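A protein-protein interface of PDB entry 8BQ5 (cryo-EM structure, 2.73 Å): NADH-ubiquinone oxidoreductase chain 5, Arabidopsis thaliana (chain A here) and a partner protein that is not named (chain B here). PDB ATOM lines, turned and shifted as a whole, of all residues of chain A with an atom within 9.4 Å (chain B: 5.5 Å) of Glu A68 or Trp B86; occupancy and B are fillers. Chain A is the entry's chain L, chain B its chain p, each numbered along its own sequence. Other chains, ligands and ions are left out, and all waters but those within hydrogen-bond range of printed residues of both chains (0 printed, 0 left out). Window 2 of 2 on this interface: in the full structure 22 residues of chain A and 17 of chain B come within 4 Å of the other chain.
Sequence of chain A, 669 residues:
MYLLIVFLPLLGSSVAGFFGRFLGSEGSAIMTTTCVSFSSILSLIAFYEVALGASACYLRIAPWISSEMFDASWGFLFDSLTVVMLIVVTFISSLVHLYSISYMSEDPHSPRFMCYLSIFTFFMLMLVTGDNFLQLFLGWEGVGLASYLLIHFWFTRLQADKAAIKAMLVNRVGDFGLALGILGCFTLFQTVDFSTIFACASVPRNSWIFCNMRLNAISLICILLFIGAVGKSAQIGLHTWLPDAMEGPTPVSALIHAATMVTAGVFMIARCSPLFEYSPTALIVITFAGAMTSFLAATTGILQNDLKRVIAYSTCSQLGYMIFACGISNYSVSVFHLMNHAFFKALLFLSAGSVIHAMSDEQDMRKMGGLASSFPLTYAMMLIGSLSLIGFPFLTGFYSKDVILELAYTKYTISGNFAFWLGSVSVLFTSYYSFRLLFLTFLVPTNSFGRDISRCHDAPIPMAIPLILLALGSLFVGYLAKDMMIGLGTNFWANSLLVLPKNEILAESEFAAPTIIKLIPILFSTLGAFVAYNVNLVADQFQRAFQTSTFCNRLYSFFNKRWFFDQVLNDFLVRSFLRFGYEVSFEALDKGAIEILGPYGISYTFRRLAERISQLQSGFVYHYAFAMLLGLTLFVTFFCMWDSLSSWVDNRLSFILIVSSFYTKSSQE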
ATOM      1  N   ILE A  65       5.880 -37.091  26.495  1.00  0.00           N
ATOM      2  CA  ILE A  65       5.593 -35.852  25.778  1.00  0.00           C
ATOM      3  C   ILE A  65       4.999 -34.882  26.789  1.00  0.00           C
ATOM      4  O   ILE A  65       3.798 -34.937  27.080  1.00  0.00           O
ATOM      5  CB  ILE A  65       4.643 -36.061  24.595  1.00  0.00           C
ATOM      6  CG1 ILE A  65       5.146 -37.184  23.688  1.00  0.00           C
ATOM      7  CG2 ILE A  65       4.487 -34.770  23.810  1.00  0.00           C
ATOM      8  CD1 ILE A  65       4.046 -37.918  22.962  1.00  0.00           C
ATOM      9  N   SER A  66       5.829 -33.995  27.327  1.00  0.00           N
ATOM     10  CA  SER A  66       5.393 -32.978  28.278  1.00  0.00           C
ATOM     11  C   SER A  66       5.507 -31.614  27.610  1.00  0.00           C
ATOM     12  O   SER A  66       6.615 -31.123  27.370  1.00  0.00           O
ATOM     13  CB  SER A  66       6.219 -33.037  29.559  1.00  0.00           C
ATOM     14  OG  SER A  66       5.491 -32.506  30.651  1.00  0.00           O
ATOM     15  N   SER A  67       4.360 -31.001  27.320  1.00  0.00           N
ATOM     16  CA  SER A  67       4.305 -29.688  26.679  1.00  0.00           C
ATOM     17  C   SER A  67       3.105 -28.950  27.262  1.00  0.00           C
ATOM     18  O   SER A  67       1.968 -29.181  26.842  1.00  0.00           O
ATOM     19  CB  SER A  67       4.203 -29.818  25.165  1.00  0.00           C
ATOM     20  OG  SER A  67       4.222 -28.547  24.542  1.00  0.00           O
ATOM     21  N   GLU A  68       3.367 -28.074  28.230  1.00  0.00           N
ATOM     22  CA  GLU A  68       2.330 -27.327  28.956  1.00  0.00           C
ATOM     23  C   GLU A  68       1.424 -28.353  29.637  1.00  0.00           C
ATOM     24  O   GLU A  68       1.912 -29.134  30.470  1.00  0.00           O
ATOM     25  CB  GLU A  68       1.634 -26.357  28.007  1.00  0.00           C
ATOM     26  CG  GLU A  68       0.811 -25.286  28.706  1.00  0.00           C
ATOM     27  CD  GLU A  68      -0.428 -24.899  27.919  1.00  0.00           C
ATOM     28  OE1 GLU A  68      -1.430 -25.638  27.988  1.00  0.00           O
ATOM     29  OE2 GLU A  68      -0.403 -23.854  27.238  1.00  0.00           O
ATOM     30  N   MET A  69       0.130 -28.401  29.322  1.00  0.00           N
ATOM     31  CA  MET A  69      -0.770 -29.305  30.027  1.00  0.00           C
ATOM     32  C   MET A  69      -0.733 -30.714  29.448  1.00  0.00           C
ATOM     33  O   MET A  69      -1.241 -31.649  30.075  1.00  0.00           O
ATOM     34  CB  MET A  69      -2.195 -28.756  29.983  1.00  0.00           C
ATOM     35  CG  MET A  69      -2.352 -27.383  30.620  1.00  0.00           C
ATOM     36  SD  MET A  69      -2.325 -27.348  32.426  1.00  0.00           S
ATOM     37  CE  MET A  69      -2.860 -29.002  32.846  1.00  0.00           C
ATOM     38  N   PHE A  70      -0.144 -30.886  28.266  1.00  0.00           N
ATOM     39  CA  PHE A  70      -0.083 -32.198  27.632  1.00  0.00           C
ATOM     40  C   PHE A  70       0.938 -33.074  28.347  1.00  0.00           C
ATOM     41  O   PHE A  70       2.125 -32.742  28.400  1.00  0.00           O
ATOM     42  CB  PHE A  70       0.269 -32.042  26.154  1.00  0.00           C
ATOM     43  CG  PHE A  70       0.014 -33.273  25.332  1.00  0.00           C
ATOM     44  CD1 PHE A  70       1.059 -34.106  24.970  1.00  0.00           C
ATOM     45  CD2 PHE A  70      -1.268 -33.596  24.920  1.00  0.00           C
ATOM     46  CE1 PHE A  70       0.830 -35.239  24.212  1.00  0.00           C
ATOM     47  CE2 PHE A  70      -1.504 -34.727  24.164  1.00  0.00           C
ATOM     48  CZ  PHE A  70      -0.453 -35.550  23.809  1.00  0.00           C
ATOM     49  N   ASP A  71       0.476 -34.205  28.879  1.00  0.00           N
ATOM     50  CA  ASP A  71       1.203 -34.956  29.897  1.00  0.00           C
ATOM     51  C   ASP A  71       1.329 -36.429  29.536  1.00  0.00           C
ATOM     52  O   ASP A  71       1.163 -37.307  30.388  1.00  0.00           O
ATOM     53  CB  ASP A  71       0.515 -34.812  31.250  1.00  0.00           C
ATOM     54  CG  ASP A  71      -0.924 -35.295  31.219  1.00  0.00           C
ATOM     55  OD1 ASP A  71      -1.543 -35.247  30.136  1.00  0.00           O
ATOM     56  OD2 ASP A  71      -1.435 -35.731  32.271  1.00  0.00           O
ATOM     57  N   ALA A  72       1.628 -36.735  28.279  1.00  0.00           N
ATOM     58  CA  ALA A  72       1.851 -38.126  27.906  1.00  0.00           C
ATOM     59  C   ALA A  72       3.146 -38.632  28.530  1.00  0.00           C
ATOM     60  O   ALA A  72       4.170 -37.946  28.518  1.00  0.00           O
ATOM     61  CB  ALA A  72       1.900 -38.271  26.387  1.00  0.00           C
ATOM     62  N   PHE A 186      -8.055 -34.521  25.190  1.00  0.00           N
ATOM     63  CA  PHE A 186      -7.148 -33.550  25.789  1.00  0.00           C
ATOM     64  C   PHE A 186      -7.764 -32.160  25.813  1.00  0.00           C
ATOM     65  O   PHE A 186      -7.631 -31.434  26.800  1.00  0.00           O
ATOM     66  CB  PHE A 186      -5.820 -33.511  25.038  1.00  0.00           C
ATOM     67  CG  PHE A 186      -4.922 -32.395  25.485  1.00  0.00           C
ATOM     68  CD1 PHE A 186      -4.271 -32.464  26.703  1.00  0.00           C
ATOM     69  CD2 PHE A 186      -4.758 -31.261  24.706  1.00  0.00           C
ATOM     70  CE1 PHE A 186      -3.457 -31.435  27.126  1.00  0.00           C
ATOM     71  CE2 PHE A 186      -3.944 -30.229  25.128  1.00  0.00           C
ATOM     72  CZ  PHE A 186      -3.292 -30.317  26.338  1.00  0.00           C
ATOM     73  N   GLN A 190      -7.798 -31.246  29.287  1.00  0.00           N
ATOM     74  CA  GLN A 190      -6.407 -30.800  29.411  1.00  0.00           C
ATOM     75  C   GLN A 190      -5.514 -31.883  30.012  1.00  0.00           C
ATOM     76  O   GLN A 190      -4.563 -31.585  30.738  1.00  0.00           O
ATOM     77  CB  GLN A 190      -6.300 -29.496  30.207  1.00  0.00           C
ATOM     78  CG  GLN A 190      -6.852 -28.289  29.463  1.00  0.00           C
ATOM     79  CD  GLN A 190      -6.088 -27.990  28.184  1.00  0.00           C
ATOM     80  OE1 GLN A 190      -4.938 -27.554  28.220  1.00  0.00           O
ATOM     81  NE2 GLN A 190      -6.727 -28.229  27.046  1.00  0.00           N
ATOM     82  N   THR A 191      -5.810 -33.143  29.702  1.00  0.00           N
ATOM     83  CA  THR A 191      -4.969 -34.260  30.104  1.00  0.00           C
ATOM     84  C   THR A 191      -5.329 -35.470  29.256  1.00  0.00           C
ATOM     85  O   THR A 191      -6.448 -35.586  28.749  1.00  0.00           O
ATOM     86  CB  THR A 191      -5.125 -34.590  31.592  1.00  0.00           C
ATOM     87  OG1 THR A 191      -4.155 -35.574  31.970  1.00  0.00           O
ATOM     88  CG2 THR A 191      -6.516 -35.131  31.877  1.00  0.00           C
ATOM     89  N   ILE B  37       4.485 -11.940  32.530  1.00  0.00           N
ATOM     90  CA  ILE B  37       3.216 -12.602  32.244  1.00  0.00           C
ATOM     91  C   ILE B  37       3.445 -14.070  31.908  1.00  0.00           C
ATOM     92  O   ILE B  37       2.680 -14.946  32.331  1.00  0.00           O
ATOM     93  CB  ILE B  37       2.473 -11.865  31.115  1.00  0.00           C
ATOM     94  CG1 ILE B  37       1.922 -10.535  31.625  1.00  0.00           C
ATOM     95  CG2 ILE B  37       1.326 -12.697  30.597  1.00  0.00           C
ATOM     96  CD1 ILE B  37       1.506  -9.595  30.523  1.00  0.00           C
ATOM     97  N   VAL B  38       4.503 -14.364  31.148  1.00  0.00           N
ATOM     98  CA  VAL B  38       4.809 -15.750  30.803  1.00  0.00           C
ATOM     99  C   VAL B  38       5.106 -16.558  32.059  1.00  0.00           C
ATOM    100  O   VAL B  38       4.598 -17.673  32.234  1.00  0.00           O
ATOM    101  CB  VAL B  38       5.981 -15.803  29.805  1.00  0.00           C
ATOM    102  CG1 VAL B  38       6.703 -17.136  29.895  1.00  0.00           C
ATOM    103  CG2 VAL B  38       5.488 -15.553  28.394  1.00  0.00           C
ATOM    104  N   LYS B  41       1.918 -17.220  33.998  1.00  0.00           N
ATOM    105  CA  LYS B  41       1.089 -18.248  33.379  1.00  0.00           C
ATOM    106  C   LYS B  41       1.664 -19.637  33.613  1.00  0.00           C
ATOM    107  O   LYS B  41       0.916 -20.610  33.755  1.00  0.00           O
ATOM    108  CB  LYS B  41       0.937 -17.974  31.884  1.00  0.00           C
ATOM    109  CG  LYS B  41      -0.063 -16.882  31.555  1.00  0.00           C
ATOM    110  CD  LYS B  41      -0.246 -16.748  30.055  1.00  0.00           C
ATOM    111  CE  LYS B  41      -1.359 -15.779  29.712  1.00  0.00           C
ATOM    112  NZ  LYS B  41      -1.911 -16.039  28.355  1.00  0.00           N
ATOM    113  N   TRP B  42       2.992 -19.752  33.654  1.00  0.00           N
ATOM    114  CA  TRP B  42       3.604 -21.054  33.888  1.00  0.00           C
ATOM    115  C   TRP B  42       3.353 -21.526  35.313  1.00  0.00           C
ATOM    116  O   TRP B  42       3.238 -22.730  35.563  1.00  0.00           O
ATOM    117  CB  TRP B  42       5.099 -20.995  33.587  1.00  0.00           C
ATOM    118  CG  TRP B  42       5.410 -21.299  32.157  1.00  0.00           C
ATOM    119  CD1 TRP B  42       5.789 -20.411  31.194  1.00  0.00           C
ATOM    120  CD2 TRP B  42       5.342 -22.578  31.519  1.00  0.00           C
ATOM    121  NE1 TRP B  42       5.974 -21.060  29.999  1.00  0.00           N
ATOM    122  CE2 TRP B  42       5.706 -22.392  30.172  1.00  0.00           C
ATOM    123  CE3 TRP B  42       5.015 -23.866  31.957  1.00  0.00           C
ATOM    124  CZ2 TRP B  42       5.752 -23.443  29.258  1.00  0.00           C
ATOM    125  CZ3 TRP B  42       5.061 -24.907  31.050  1.00  0.00           C
ATOM    126  CH2 TRP B  42       5.427 -24.690  29.716  1.00  0.00           C
ATOM    127  N   ILE B  45      -0.073 -23.002  35.182  1.00  0.00           N
ATOM    128  CA  ILE B  45      -0.054 -24.308  34.528  1.00  0.00           C
ATOM    129  C   ILE B  45       0.437 -25.374  35.495  1.00  0.00           C
ATOM    130  O   ILE B  45      -0.136 -26.467  35.589  1.00  0.00           O
ATOM    131  CB  ILE B  45       0.806 -24.275  33.252  1.00  0.00           C
ATOM    132  CG1 ILE B  45       0.206 -23.339  32.207  1.00  0.00           C
ATOM    133  CG2 ILE B  45       0.951 -25.670  32.672  1.00  0.00           C
ATOM    134  CD1 ILE B  45       1.246 -22.661  31.364  1.00  0.00           C
ATOM    135  N   LYS B  49      -1.350 -28.624  37.245  1.00  0.00           N
ATOM    136  CA  LYS B  49      -0.711 -29.928  37.107  1.00  0.00           C
ATOM    137  C   LYS B  49      -0.573 -30.624  38.456  1.00  0.00           C
ATOM    138  O   LYS B  49      -0.674 -31.853  38.539  1.00  0.00           O
ATOM    139  CB  LYS B  49       0.653 -29.773  36.437  1.00  0.00           C
ATOM    140  CG  LYS B  49       0.571 -29.525  34.941  1.00  0.00           C
ATOM    141  CD  LYS B  49       1.901 -29.070  34.367  1.00  0.00           C
ATOM    142  CE  LYS B  49       2.754 -30.245  33.910  1.00  0.00           C
ATOM    143  NZ  LYS B  49       3.233 -31.089  35.038  1.00  0.00           N
ATOM    144  N   ARG B  52      -3.891 -31.813  39.254  1.00  0.00           N
ATOM    145  CA  ARG B  52      -4.203 -32.990  38.449  1.00  0.00           C
ATOM    146  C   ARG B  52      -3.674 -34.259  39.105  1.00  0.00           C
ATOM    147  O   ARG B  52      -4.302 -35.321  39.021  1.00  0.00           O
ATOM    148  CB  ARG B  52      -3.625 -32.828  37.043  1.00  0.00           C
ATOM    149  CG  ARG B  52      -3.800 -34.039  36.143  1.00  0.00           C
ATOM    150  CD  ARG B  52      -3.504 -33.684  34.699  1.00  0.00           C
ATOM    151  NE  ARG B  52      -2.095 -33.366  34.504  1.00  0.00           N
ATOM    152  CZ  ARG B  52      -1.613 -32.706  33.461  1.00  0.00           C
ATOM    153  NH1 ARG B  52      -2.399 -32.291  32.481  1.00  0.00           N
ATOM    154  NH2 ARG B  52      -0.309 -32.456  33.398  1.00  0.00           N
ATOM    155  N   VAL B  84      -6.270 -21.455  31.498  1.00  0.00           N
ATOM    156  CA  VAL B  84      -4.919 -21.854  31.865  1.00  0.00           C
ATOM    157  C   VAL B  84      -4.091 -21.984  30.595  1.00  0.00           C
ATOM    158  O   VAL B  84      -4.598 -22.355  29.531  1.00  0.00           O
ATOM    159  CB  VAL B  84      -4.891 -23.170  32.679  1.00  0.00           C
ATOM    160  CG1 VAL B  84      -5.009 -24.386  31.772  1.00  0.00           C
ATOM    161  CG2 VAL B  84      -3.626 -23.252  33.512  1.00  0.00           C
ATOM    162  N   GLY B  85      -2.810 -21.648  30.713  1.00  0.00           N
ATOM    163  CA  GLY B  85      -1.896 -21.730  29.594  1.00  0.00           C
ATOM    164  C   GLY B  85      -2.337 -20.919  28.396  1.00  0.00           C
ATOM    165  O   GLY B  85      -2.745 -19.762  28.529  1.00  0.00           O
ATOM    166  N   TRP B  86      -2.277 -21.531  27.217  1.00  0.00           N
ATOM    167  CA  TRP B  86      -2.570 -20.853  25.963  1.00  0.00           C
ATOM    168  C   TRP B  86      -3.557 -21.654  25.119  1.00  0.00           C
ATOM    169  O   TRP B  86      -3.548 -21.573  23.890  1.00  0.00           O
ATOM    170  CB  TRP B  86      -1.275 -20.586  25.198  1.00  0.00           C
ATOM    171  CG  TRP B  86      -0.394 -19.553  25.855  1.00  0.00           C
ATOM    172  CD1 TRP B  86      -0.357 -18.221  25.581  1.00  0.00           C
ATOM    173  CD2 TRP B  86       0.565 -19.773  26.899  1.00  0.00           C
ATOM    174  NE1 TRP B  86       0.570 -17.596  26.379  1.00  0.00           N
ATOM    175  CE2 TRP B  86       1.148 -18.527  27.200  1.00  0.00           C
ATOM    176  CE3 TRP B  86       0.986 -20.901  27.609  1.00  0.00           C
ATOM    177  CZ2 TRP B  86       2.132 -18.377  28.174  1.00  0.00           C
ATOM    178  CZ3 TRP B  86       1.964 -20.748  28.575  1.00  0.00           C
ATOM    179  CH2 TRP B  86       2.522 -19.497  28.851  1.00  0.00           C
ATOM    180  N   GLY B  87      -4.425 -22.419  25.777  1.00  0.00           N
ATOM    181  CA  GLY B  87      -5.376 -23.275  25.093  1.00  0.00           C
ATOM    182  C   GLY B  87      -6.622 -22.557  24.617  1.00  0.00           C
ATOM    183  O   GLY B  87      -6.533 -21.497  23.992  1.00  0.00           O
ATOM    184  N   LYS B  88      -7.793 -23.116  24.916  1.00  0.00           N
ATOM    185  CA  LYS B  88      -9.048 -22.646  24.346  1.00  0.00           C
ATOM    186  C   LYS B  88      -9.664 -21.477  25.107  1.00  0.00           C
ATOM    187  O   LYS B  88     -10.749 -21.021  24.735  1.00  0.00           O
ATOM    188  CB  LYS B  88     -10.058 -23.791  24.268  1.00  0.00           C
ATOM    189  CG  LYS B  88     -10.124 -24.433  22.899  1.00  0.00           C
ATOM    190  CD  LYS B  88     -11.296 -25.383  22.777  1.00  0.00           C
ATOM    191  CE  LYS B  88     -12.612 -24.633  22.820  1.00  0.00           C
ATOM    192  NZ  LYS B  88     -13.592 -25.196  21.853  1.00  0.00           N
ATOM    193  N   ASP B  89      -9.016 -20.989  26.159  1.00  0.00           N
ATOM    194  CA  ASP B  89      -9.520 -19.831  26.883  1.00  0.00           C
ATOM    195  C   ASP B  89      -8.539 -18.678  26.739  1.00  0.00           C
ATOM    196  O   ASP B  89      -7.323 -18.877  26.783  1.00  0.00           O
ATOM    197  CB  ASP B  89      -9.753 -20.140  28.364  1.00  0.00           C
ATOM    198  CG  ASP B  89     -10.853 -21.164  28.583  1.00  0.00           C
ATOM    199  OD1 ASP B  89     -11.166 -21.922  27.643  1.00  0.00           O
ATOM    200  OD2 ASP B  89     -11.411 -21.203  29.699  1.00  0.00           O
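The side-chain carboxylate (OE2) of Glu A68 lies within hydrogen-bond range of the backbone NH (N) of Trp B86 (3.0 Å). The backbone carbonyl oxygen (O) of Met A69 is in hydrogen-bond range of the guanidinium group (NH1) of Arg B52 (2.7 Å). The side-chain carboxylate (OD2) of Asp A71 lies within salt-bridge range of the guanidinium group (NE) of Arg B52 (3.3 Å). The backbone carbonyl oxygen of Gln A190 sits at hydrogen-bond distance from the guanidinium group of Arg B52 (2.9 Å).
The side-chain hydroxyl (OG1) of Thr A191 is in hydrogen-bond range of the side-chain carboxylate (OD2) of Asp A71, at 2.7 Å. O of Phe A186 sits close to NE2 of Gln A190, 3.3 Å away.
Ile B45 touches Glu A68 (CD1 to CG, 3.8 Å). CE of Lys B49 touches O of Glu A68, at 3.7 Å. Glu A68 touches Gly B85. SD of Met A69 touches CG2 of Ile B45, 3.7 Å away. CD of Arg B52 touches OG1 of Thr A191 (3.4 Å).
Of chain B, only Ile B45 (3.8 Å), Lys B49 (3.7 Å), Gly B85 (3.5 Å) and Trp B86 (3.0 Å) come within 4 Å of Glu A68. Trp B86 touches one residue of chain A. Gly B85 touches just one residue of chain A: Glu A68 (3.5 Å). Of the printed residues of chain B, Asp A71 touches Arg B52 (3.3 Å). Printed residues of chain A within 4 Å of Ile B45: Glu A68 and Met A69. Printed residues of chain B within 4 Å of Gln A190: Arg B52. Of the printed residues of chain A, Lys B49 touches Glu A68 (3.7 Å). Of the printed residues of chain B, Thr A191 touches Arg B52 (3.4 Å). Asp B89 touches none of the printed residues of chain A. Ile A65 touches none of the printed residues of chain B. The nearest printed residue of chain B that does not touch Met A69 is Val B84 (4.1 Å).
Of the 11 printed residues of chain A, 5 touch a printed residue of chain B. Of the 13 printed residues of chain B, 5 touch a printed residue of chain A. Among the printed residues, Asp or Glu carboxylates within 4 Å of a Lys or Arg side-chain nitrogen of the other chain: Asp A71 with Arg B52.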
